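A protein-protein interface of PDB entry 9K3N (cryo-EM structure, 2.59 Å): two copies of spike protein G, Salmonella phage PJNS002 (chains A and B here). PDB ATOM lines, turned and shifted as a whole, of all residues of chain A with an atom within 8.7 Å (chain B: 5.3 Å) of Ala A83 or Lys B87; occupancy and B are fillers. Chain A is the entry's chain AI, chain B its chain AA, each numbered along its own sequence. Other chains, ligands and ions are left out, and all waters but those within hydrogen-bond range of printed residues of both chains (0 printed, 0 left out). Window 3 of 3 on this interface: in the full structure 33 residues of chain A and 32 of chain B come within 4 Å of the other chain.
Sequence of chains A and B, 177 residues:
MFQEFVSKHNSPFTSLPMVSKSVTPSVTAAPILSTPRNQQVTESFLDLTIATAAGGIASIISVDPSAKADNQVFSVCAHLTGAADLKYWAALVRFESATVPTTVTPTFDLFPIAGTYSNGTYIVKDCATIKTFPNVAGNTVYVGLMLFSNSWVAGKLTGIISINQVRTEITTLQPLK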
ATOM      1  N   ASP A  47     -23.079  20.996  15.490  1.00  0.00           N
ATOM      2  CA  ASP A  47     -22.584  19.943  16.373  1.00  0.00           C
ATOM      3  C   ASP A  47     -23.652  19.683  17.424  1.00  0.00           C
ATOM      4  O   ASP A  47     -23.918  20.548  18.261  1.00  0.00           O
ATOM      5  CB  ASP A  47     -21.256  20.337  17.017  1.00  0.00           C
ATOM      6  CG  ASP A  47     -20.062  20.029  16.132  1.00  0.00           C
ATOM      7  OD1 ASP A  47     -20.069  18.978  15.460  1.00  0.00           O
ATOM      8  OD2 ASP A  47     -19.122  20.848  16.088  1.00  0.00           O
ATOM      9  N   HIS A  79     -31.359  14.543   6.780  1.00  0.00           N
ATOM     10  CA  HIS A  79     -30.112  13.897   6.411  1.00  0.00           C
ATOM     11  C   HIS A  79     -29.142  14.022   7.570  1.00  0.00           C
ATOM     12  O   HIS A  79     -28.234  14.852   7.545  1.00  0.00           O
ATOM     13  CB  HIS A  79     -29.532  14.532   5.152  1.00  0.00           C
ATOM     14  CG  HIS A  79     -28.352  13.803   4.591  1.00  0.00           C
ATOM     15  ND1 HIS A  79     -27.463  13.103   5.379  1.00  0.00           N
ATOM     16  CD2 HIS A  79     -27.910  13.671   3.318  1.00  0.00           C
ATOM     17  CE1 HIS A  79     -26.525  12.571   4.615  1.00  0.00           C
ATOM     18  NE2 HIS A  79     -26.774  12.900   3.360  1.00  0.00           N
ATOM     19  N   LEU A  80     -29.338  13.201   8.591  1.00  0.00           N
ATOM     20  CA  LEU A  80     -28.473  13.263   9.758  1.00  0.00           C
ATOM     21  C   LEU A  80     -27.257  12.384   9.555  1.00  0.00           C
ATOM     22  O   LEU A  80     -27.366  11.275   9.030  1.00  0.00           O
ATOM     23  CB  LEU A  80     -29.240  12.836  11.004  1.00  0.00           C
ATOM     24  CG  LEU A  80     -30.475  13.698  11.264  1.00  0.00           C
ATOM     25  CD1 LEU A  80     -31.007  13.450  12.665  1.00  0.00           C
ATOM     26  CD2 LEU A  80     -30.144  15.170  11.059  1.00  0.00           C
ATOM     27  N   THR A  81     -26.095  12.874   9.971  1.00  0.00           N
ATOM     28  CA  THR A  81     -24.867  12.114   9.772  1.00  0.00           C
ATOM     29  C   THR A  81     -23.890  12.474  10.885  1.00  0.00           C
ATOM     30  O   THR A  81     -24.190  13.289  11.761  1.00  0.00           O
ATOM     31  CB  THR A  81     -24.256  12.387   8.393  1.00  0.00           C
ATOM     32  OG1 THR A  81     -23.083  11.584   8.223  1.00  0.00           O
ATOM     33  CG2 THR A  81     -23.881  13.854   8.263  1.00  0.00           C
ATOM     34  N   GLY A  82     -22.715  11.863  10.837  1.00  0.00           N
ATOM     35  CA  GLY A  82     -21.707  12.125  11.843  1.00  0.00           C
ATOM     36  C   GLY A  82     -20.381  11.508  11.461  1.00  0.00           C
ATOM     37  O   GLY A  82     -20.182  11.066  10.328  1.00  0.00           O
ATOM     38  N   ALA A  83     -19.470  11.484  12.431  1.00  0.00           N
ATOM     39  CA  ALA A  83     -18.139  10.924  12.225  1.00  0.00           C
ATOM     40  C   ALA A  83     -18.015   9.478  12.682  1.00  0.00           C
ATOM     41  O   ALA A  83     -17.143   8.759  12.186  1.00  0.00           O
ATOM     42  CB  ALA A  83     -17.087  11.771  12.953  1.00  0.00           C
ATOM     43  N   ALA A  84     -18.860   9.039  13.611  1.00  0.00           N
ATOM     44  CA  ALA A  84     -18.835   7.677  14.125  1.00  0.00           C
ATOM     45  C   ALA A  84     -20.240   7.091  14.067  1.00  0.00           C
ATOM     46  O   ALA A  84     -21.205   7.760  13.682  1.00  0.00           O
ATOM     47  CB  ALA A  84     -18.279   7.632  15.553  1.00  0.00           C
ATOM     48  N   ASP A  85     -20.352   5.826  14.461  1.00  0.00           N
ATOM     49  CA  ASP A  85     -21.623   5.116  14.475  1.00  0.00           C
ATOM     50  C   ASP A  85     -22.228   5.210  15.874  1.00  0.00           C
ATOM     51  O   ASP A  85     -21.589   4.810  16.855  1.00  0.00           O
ATOM     52  CB  ASP A  85     -21.424   3.659  14.063  1.00  0.00           C
ATOM     53  CG  ASP A  85     -22.716   2.981  13.656  1.00  0.00           C
ATOM     54  OD1 ASP A  85     -23.801   3.478  14.021  1.00  0.00           O
ATOM     55  OD2 ASP A  85     -22.644   1.940  12.969  1.00  0.00           O
ATOM     56  N   LEU A  86     -23.448   5.735  15.962  1.00  0.00           N
ATOM     57  CA  LEU A  86     -24.118   5.930  17.242  1.00  0.00           C
ATOM     58  C   LEU A  86     -25.228   4.916  17.501  1.00  0.00           C
ATOM     59  O   LEU A  86     -25.814   4.933  18.590  1.00  0.00           O
ATOM     60  CB  LEU A  86     -24.679   7.353  17.328  1.00  0.00           C
ATOM     61  CG  LEU A  86     -23.657   8.485  17.167  1.00  0.00           C
ATOM     62  CD1 LEU A  86     -24.274   9.826  17.534  1.00  0.00           C
ATOM     63  CD2 LEU A  86     -22.409   8.222  17.998  1.00  0.00           C
ATOM     64  N   ASN A 119     -24.128   3.371   7.662  1.00  0.00           N
ATOM     65  CA  ASN A 119     -23.350   3.136   8.876  1.00  0.00           C
ATOM     66  C   ASN A 119     -23.831   3.989  10.038  1.00  0.00           C
ATOM     67  O   ASN A 119     -24.185   3.446  11.090  1.00  0.00           O
ATOM     68  CB  ASN A 119     -21.860   3.382   8.604  1.00  0.00           C
ATOM     69  CG  ASN A 119     -21.143   2.135   8.135  1.00  0.00           C
ATOM     70  OD1 ASN A 119     -21.334   1.053   8.687  1.00  0.00           O
ATOM     71  ND2 ASN A 119     -20.315   2.278   7.106  1.00  0.00           N
ATOM     72  N   GLY A 120     -23.869   5.307   9.879  1.00  0.00           N
ATOM     73  CA  GLY A 120     -24.384   6.188  10.906  1.00  0.00           C
ATOM     74  C   GLY A 120     -25.131   7.355  10.298  1.00  0.00           C
ATOM     75  O   GLY A 120     -25.533   8.287  11.002  1.00  0.00           O
ATOM     76  N   THR A 121     -25.313   7.310   8.983  1.00  0.00           N
ATOM     77  CA  THR A 121     -26.020   8.345   8.243  1.00  0.00           C
ATOM     78  C   THR A 121     -27.450   7.888   7.992  1.00  0.00           C
ATOM     79  O   THR A 121     -27.675   6.763   7.536  1.00  0.00           O
ATOM     80  CB  THR A 121     -25.321   8.644   6.917  1.00  0.00           C
ATOM     81  OG1 THR A 121     -23.967   9.047   7.166  1.00  0.00           O
ATOM     82  CG2 THR A 121     -26.044   9.749   6.165  1.00  0.00           C
ATOM     83  N   GLY A 155     -20.902  10.866  21.367  1.00  0.00           N
ATOM     84  CA  GLY A 155     -20.400  11.414  20.124  1.00  0.00           C
ATOM     85  C   GLY A 155     -21.132  12.687  19.765  1.00  0.00           C
ATOM     86  O   GLY A 155     -21.963  13.185  20.527  1.00  0.00           O
ATOM     87  N   LYS A 156     -20.814  13.209  18.580  1.00  0.00           N
ATOM     88  CA  LYS A 156     -21.409  14.439  18.080  1.00  0.00           C
ATOM     89  C   LYS A 156     -22.041  14.186  16.717  1.00  0.00           C
ATOM     90  O   LYS A 156     -21.524  13.395  15.924  1.00  0.00           O
ATOM     91  CB  LYS A 156     -20.365  15.559  17.989  1.00  0.00           C
ATOM     92  CG  LYS A 156     -19.669  15.843  19.313  1.00  0.00           C
ATOM     93  CD  LYS A 156     -18.854  17.119  19.257  1.00  0.00           C
ATOM     94  CE  LYS A 156     -17.768  17.050  18.199  1.00  0.00           C
ATOM     95  NZ  LYS A 156     -16.680  16.100  18.531  1.00  0.00           N
ATOM     96  N   LEU A 157     -23.156  14.867  16.453  1.00  0.00           N
ATOM     97  CA  LEU A 157     -23.951  14.647  15.253  1.00  0.00           C
ATOM     98  C   LEU A 157     -24.221  15.971  14.550  1.00  0.00           C
ATOM     99  O   LEU A 157     -24.254  17.031  15.181  1.00  0.00           O
ATOM    100  CB  LEU A 157     -25.287  13.966  15.589  1.00  0.00           C
ATOM    101  CG  LEU A 157     -25.849  12.939  14.607  1.00  0.00           C
ATOM    102  CD1 LEU A 157     -24.904  11.763  14.492  1.00  0.00           C
ATOM    103  CD2 LEU A 157     -27.227  12.475  15.049  1.00  0.00           C
ATOM    104  N   THR A 158     -24.424  15.898  13.236  1.00  0.00           N
ATOM    105  CA  THR A 158     -24.714  17.079  12.434  1.00  0.00           C
ATOM    106  C   THR A 158     -25.618  16.690  11.274  1.00  0.00           C
ATOM    107  O   THR A 158     -25.583  15.554  10.794  1.00  0.00           O
ATOM    108  CB  THR A 158     -23.426  17.735  11.919  1.00  0.00           C
ATOM    109  OG1 THR A 158     -23.753  18.841  11.071  1.00  0.00           O
ATOM    110  CG2 THR A 158     -22.588  16.731  11.140  1.00  0.00           C
ATOM    111  N   ASP B  85     -13.056   8.653   3.180  1.00  0.00           N
ATOM    112  CA  ASP B  85     -14.281   9.180   3.767  1.00  0.00           C
ATOM    113  C   ASP B  85     -14.005  10.576   4.318  1.00  0.00           C
ATOM    114  O   ASP B  85     -13.111  10.751   5.153  1.00  0.00           O
ATOM    115  CB  ASP B  85     -14.786   8.248   4.868  1.00  0.00           C
ATOM    116  CG  ASP B  85     -16.235   8.498   5.230  1.00  0.00           C
ATOM    117  OD1 ASP B  85     -16.756   9.591   4.921  1.00  0.00           O
ATOM    118  OD2 ASP B  85     -16.857   7.596   5.830  1.00  0.00           O
ATOM    119  N   LEU B  86     -14.769  11.562   3.852  1.00  0.00           N
ATOM    120  CA  LEU B  86     -14.577  12.949   4.252  1.00  0.00           C
ATOM    121  C   LEU B  86     -15.638  13.446   5.229  1.00  0.00           C
ATOM    122  O   LEU B  86     -15.534  14.584   5.702  1.00  0.00           O
ATOM    123  CB  LEU B  86     -14.538  13.854   3.016  1.00  0.00           C
ATOM    124  CG  LEU B  86     -13.460  13.523   1.979  1.00  0.00           C
ATOM    125  CD1 LEU B  86     -13.347  14.630   0.944  1.00  0.00           C
ATOM    126  CD2 LEU B  86     -12.115  13.268   2.645  1.00  0.00           C
ATOM    127  N   LYS B  87     -16.647  12.629   5.539  1.00  0.00           N
ATOM    128  CA  LYS B  87     -17.630  12.897   6.593  1.00  0.00           C
ATOM    129  C   LYS B  87     -18.370  14.216   6.346  1.00  0.00           C
ATOM    130  O   LYS B  87     -18.244  15.186   7.096  1.00  0.00           O
ATOM    131  CB  LYS B  87     -16.963  12.903   7.975  1.00  0.00           C
ATOM    132  CG  LYS B  87     -15.918  11.826   8.185  1.00  0.00           C
ATOM    133  CD  LYS B  87     -16.541  10.447   8.263  1.00  0.00           C
ATOM    134  CE  LYS B  87     -15.489   9.385   8.518  1.00  0.00           C
ATOM    135  NZ  LYS B  87     -14.759   9.611   9.797  1.00  0.00           N
ATOM    136  N   TYR B  88     -19.153  14.227   5.269  1.00  0.00           N
ATOM    137  CA  TYR B  88     -19.889  15.414   4.858  1.00  0.00           C
ATOM    138  C   TYR B  88     -21.344  15.063   4.564  1.00  0.00           C
ATOM    139  O   TYR B  88     -21.714  13.894   4.438  1.00  0.00           O
ATOM    140  CB  TYR B  88     -19.242  16.068   3.627  1.00  0.00           C
ATOM    141  CG  TYR B  88     -19.233  15.195   2.390  1.00  0.00           C
ATOM    142  CD1 TYR B  88     -18.208  14.285   2.165  1.00  0.00           C
ATOM    143  CD2 TYR B  88     -20.244  15.289   1.442  1.00  0.00           C
ATOM    144  CE1 TYR B  88     -18.197  13.486   1.034  1.00  0.00           C
ATOM    145  CE2 TYR B  88     -20.239  14.495   0.310  1.00  0.00           C
ATOM    146  CZ  TYR B  88     -19.213  13.597   0.111  1.00  0.00           C
ATOM    147  OH  TYR B  88     -19.205  12.807  -1.016  1.00  0.00           O
ATOM    148  N   TRP B  89     -22.167  16.107   4.459  1.00  0.00           N
ATOM    149  CA  TRP B  89     -23.561  15.992   4.051  1.00  0.00           C
ATOM    150  C   TRP B  89     -23.904  17.191   3.172  1.00  0.00           C
ATOM    151  O   TRP B  89     -23.158  18.169   3.104  1.00  0.00           O
ATOM    152  CB  TRP B  89     -24.504  15.900   5.260  1.00  0.00           C
ATOM    153  CG  TRP B  89     -24.320  16.985   6.283  1.00  0.00           C
ATOM    154  CD1 TRP B  89     -23.377  17.034   7.266  1.00  0.00           C
ATOM    155  CD2 TRP B  89     -25.114  18.170   6.431  1.00  0.00           C
ATOM    156  NE1 TRP B  89     -23.529  18.176   8.012  1.00  0.00           N
ATOM    157  CE2 TRP B  89     -24.587  18.890   7.521  1.00  0.00           C
ATOM    158  CE3 TRP B  89     -26.216  18.692   5.747  1.00  0.00           C
ATOM    159  CZ2 TRP B  89     -25.123  20.104   7.940  1.00  0.00           C
ATOM    160  CZ3 TRP B  89     -26.747  19.898   6.165  1.00  0.00           C
ATOM    161  CH2 TRP B  89     -26.200  20.590   7.252  1.00  0.00           C
ATOM    162  N   TYR B 117     -25.785   7.802   0.699  1.00  0.00           N
ATOM    163  CA  TYR B 117     -24.427   8.028   1.195  1.00  0.00           C
ATOM    164  C   TYR B 117     -23.950   6.736   1.858  1.00  0.00           C
ATOM    165  O   TYR B 117     -24.301   6.466   3.011  1.00  0.00           O
ATOM    166  CB  TYR B 117     -24.395   9.202   2.163  1.00  0.00           C
ATOM    167  CG  TYR B 117     -23.009   9.619   2.600  1.00  0.00           C
ATOM    168  CD1 TYR B 117     -22.414   9.058   3.722  1.00  0.00           C
ATOM    169  CD2 TYR B 117     -22.297  10.578   1.892  1.00  0.00           C
ATOM    170  CE1 TYR B 117     -21.150   9.438   4.125  1.00  0.00           C
ATOM    171  CE2 TYR B 117     -21.031  10.964   2.287  1.00  0.00           C
ATOM    172  CZ  TYR B 117     -20.463  10.392   3.404  1.00  0.00           C
ATOM    173  OH  TYR B 117     -19.203  10.774   3.802  1.00  0.00           O
ATOM    174  N   PHE B 148     -21.702  20.296   3.357  1.00  0.00           N
ATOM    175  CA  PHE B 148     -21.383  20.820   4.675  1.00  0.00           C
ATOM    176  C   PHE B 148     -20.848  19.714   5.576  1.00  0.00           C
ATOM    177  O   PHE B 148     -21.273  18.558   5.490  1.00  0.00           O
ATOM    178  CB  PHE B 148     -22.612  21.467   5.323  1.00  0.00           C
ATOM    179  CG  PHE B 148     -22.275  22.486   6.374  1.00  0.00           C
ATOM    180  CD1 PHE B 148     -22.093  22.108   7.693  1.00  0.00           C
ATOM    181  CD2 PHE B 148     -22.142  23.823   6.040  1.00  0.00           C
ATOM    182  CE1 PHE B 148     -21.781  23.045   8.661  1.00  0.00           C
ATOM    183  CE2 PHE B 148     -21.832  24.763   7.002  1.00  0.00           C
ATOM    184  CZ  PHE B 148     -21.653  24.374   8.315  1.00  0.00           C
ATOM    185  N   SER B 149     -19.908  20.085   6.442  1.00  0.00           N
ATOM    186  CA  SER B 149     -19.330  19.158   7.404  1.00  0.00           C
ATOM    187  C   SER B 149     -18.846  19.938   8.616  1.00  0.00           C
ATOM    188  O   SER B 149     -18.268  21.019   8.477  1.00  0.00           O
ATOM    189  CB  SER B 149     -18.170  18.365   6.790  1.00  0.00           C
ATOM    190  OG  SER B 149     -17.619  17.462   7.731  1.00  0.00           O
ATOM    191  N   ASN B 150     -19.086  19.383   9.806  1.00  0.00           N
ATOM    192  CA  ASN B 150     -18.627  20.035  11.027  1.00  0.00           C
ATOM    193  C   ASN B 150     -17.124  19.896  11.224  1.00  0.00           C
ATOM    194  O   ASN B 150     -16.529  20.699  11.950  1.00  0.00           O
ATOM    195  CB  ASN B 150     -19.370  19.471  12.240  1.00  0.00           C
ATOM    196  CG  ASN B 150     -19.144  17.983  12.424  1.00  0.00           C
ATOM    197  OD1 ASN B 150     -18.808  17.272  11.478  1.00  0.00           O
ATOM    198  ND2 ASN B 150     -19.336  17.502  13.647  1.00  0.00           N
ATOM    199  N   SER B 151     -16.497  18.896  10.599  1.00  0.00           N
ATOM    200  CA  SER B 151     -15.044  18.743  10.663  1.00  0.00           C
ATOM    201  C   SER B 151     -14.615  17.976   9.413  1.00  0.00           C
ATOM    202  O   SER B 151     -14.740  16.749   9.366  1.00  0.00           O
ATOM    203  CB  SER B 151     -14.618  18.024  11.933  1.00  0.00           C
ATOM    204  OG  SER B 151     -14.940  18.784  13.084  1.00  0.00           O
ATOM    205  N   VAL B 153     -12.195  16.292   6.527  1.00  0.00           N
ATOM    206  CA  VAL B 153     -10.978  15.490   6.499  1.00  0.00           C
ATOM    207  C   VAL B 153     -10.218  15.844   5.230  1.00  0.00           C
ATOM    208  O   VAL B 153     -10.804  15.893   4.144  1.00  0.00           O
ATOM    209  CB  VAL B 153     -11.290  13.984   6.557  1.00  0.00           C
ATOM    210  CG1 VAL B 153     -10.009  13.171   6.497  1.00  0.00           C
ATOM    211  CG2 VAL B 153     -12.081  13.654   7.814  1.00  0.00           C
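Among the printed residues, pairs that only touch across the chains: His A79 with Trp B89 (3.9 Å), Thr A81 with Trp B89 (3.4 Å), Thr A121 with Tyr B117 (3.8 Å) and Thr A158 with Asn B150 (3.8 Å).
2 positions are printed for both chains.
Of the 7 pairs that touch across the chains among the printed residues, none has its exchanged pair printed and touching as well.
The side-chain hydroxyl (OG1) of Thr A158 sits at hydrogen-bond distance from the indole nitrogen (NE1) of Trp B89.
The side-chain amide nitrogen (ND2) of Asn B150 sits at hydrogen-bond distance from the side-chain carboxylate (OD1) of Asp A47 (2.5 Å).
The side-chain amino group of Lys B87 sits at hydrogen-bond distance from the backbone carbonyl oxygen of Ala A83.
The backbone NH of Thr A81 sits at hydrogen-bond distance from the backbone carbonyl oxygen of Thr A158.
The backbone NH of Lys B87 sits at hydrogen-bond distance from the side-chain carboxylate of Asp B85 (3.1 Å).
The side-chain hydroxyl of Thr A81 sits at hydrogen-bond distance from the side-chain hydroxyl of Thr A121 (2.9 Å).
N of Phe B148 is in hydrogen-bond range of O of Trp B89 (2.6 Å).
OG of Ser B149 sits at hydrogen-bond distance from O of Lys B87 (2.4 Å).
The side-chain carboxylate of Asp B85 lies within hydrogen-bond range of the side-chain hydroxyl of Tyr B117, at 2.9 Å.
Of the printed residues of chain B, Thr A81 touches Trp B89 (3.4 Å).
Ala A83 touches just one residue of chain B: Lys B87 (3.5 Å).
Of the printed residues of chain B, Thr A121 touches Tyr B117.
Of chain A, only Ala A83 (3.5 Å) comes within 4 Å of Lys B87.
The nearest printed residue of chain B that does not touch Ala A83 is Asn B150 (5.9 Å).
The nearest printed residue of chain B that does not touch Thr A121 is Tyr B88 (6.0 Å).
Of the 16 printed residues of chain A, 6 touch a printed residue of chain B.
Printed residues of chain A that touch a printed residue of chain B: Asp A47, His A79, Thr A81, Ala A83, Thr A121 and Thr A158.
Hydrophobic or aromatic side chains of chain A that line the printed part of chain B: His A79.
Printed residues of chain B that touch a printed residue of chain A: Lys B87, Trp B89, Tyr B117 and Asn B150.
Among the printed residues, no Asp or Glu carboxylate lies within 4 Å of a Lys or Arg side-chain nitrogen of the other chain.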
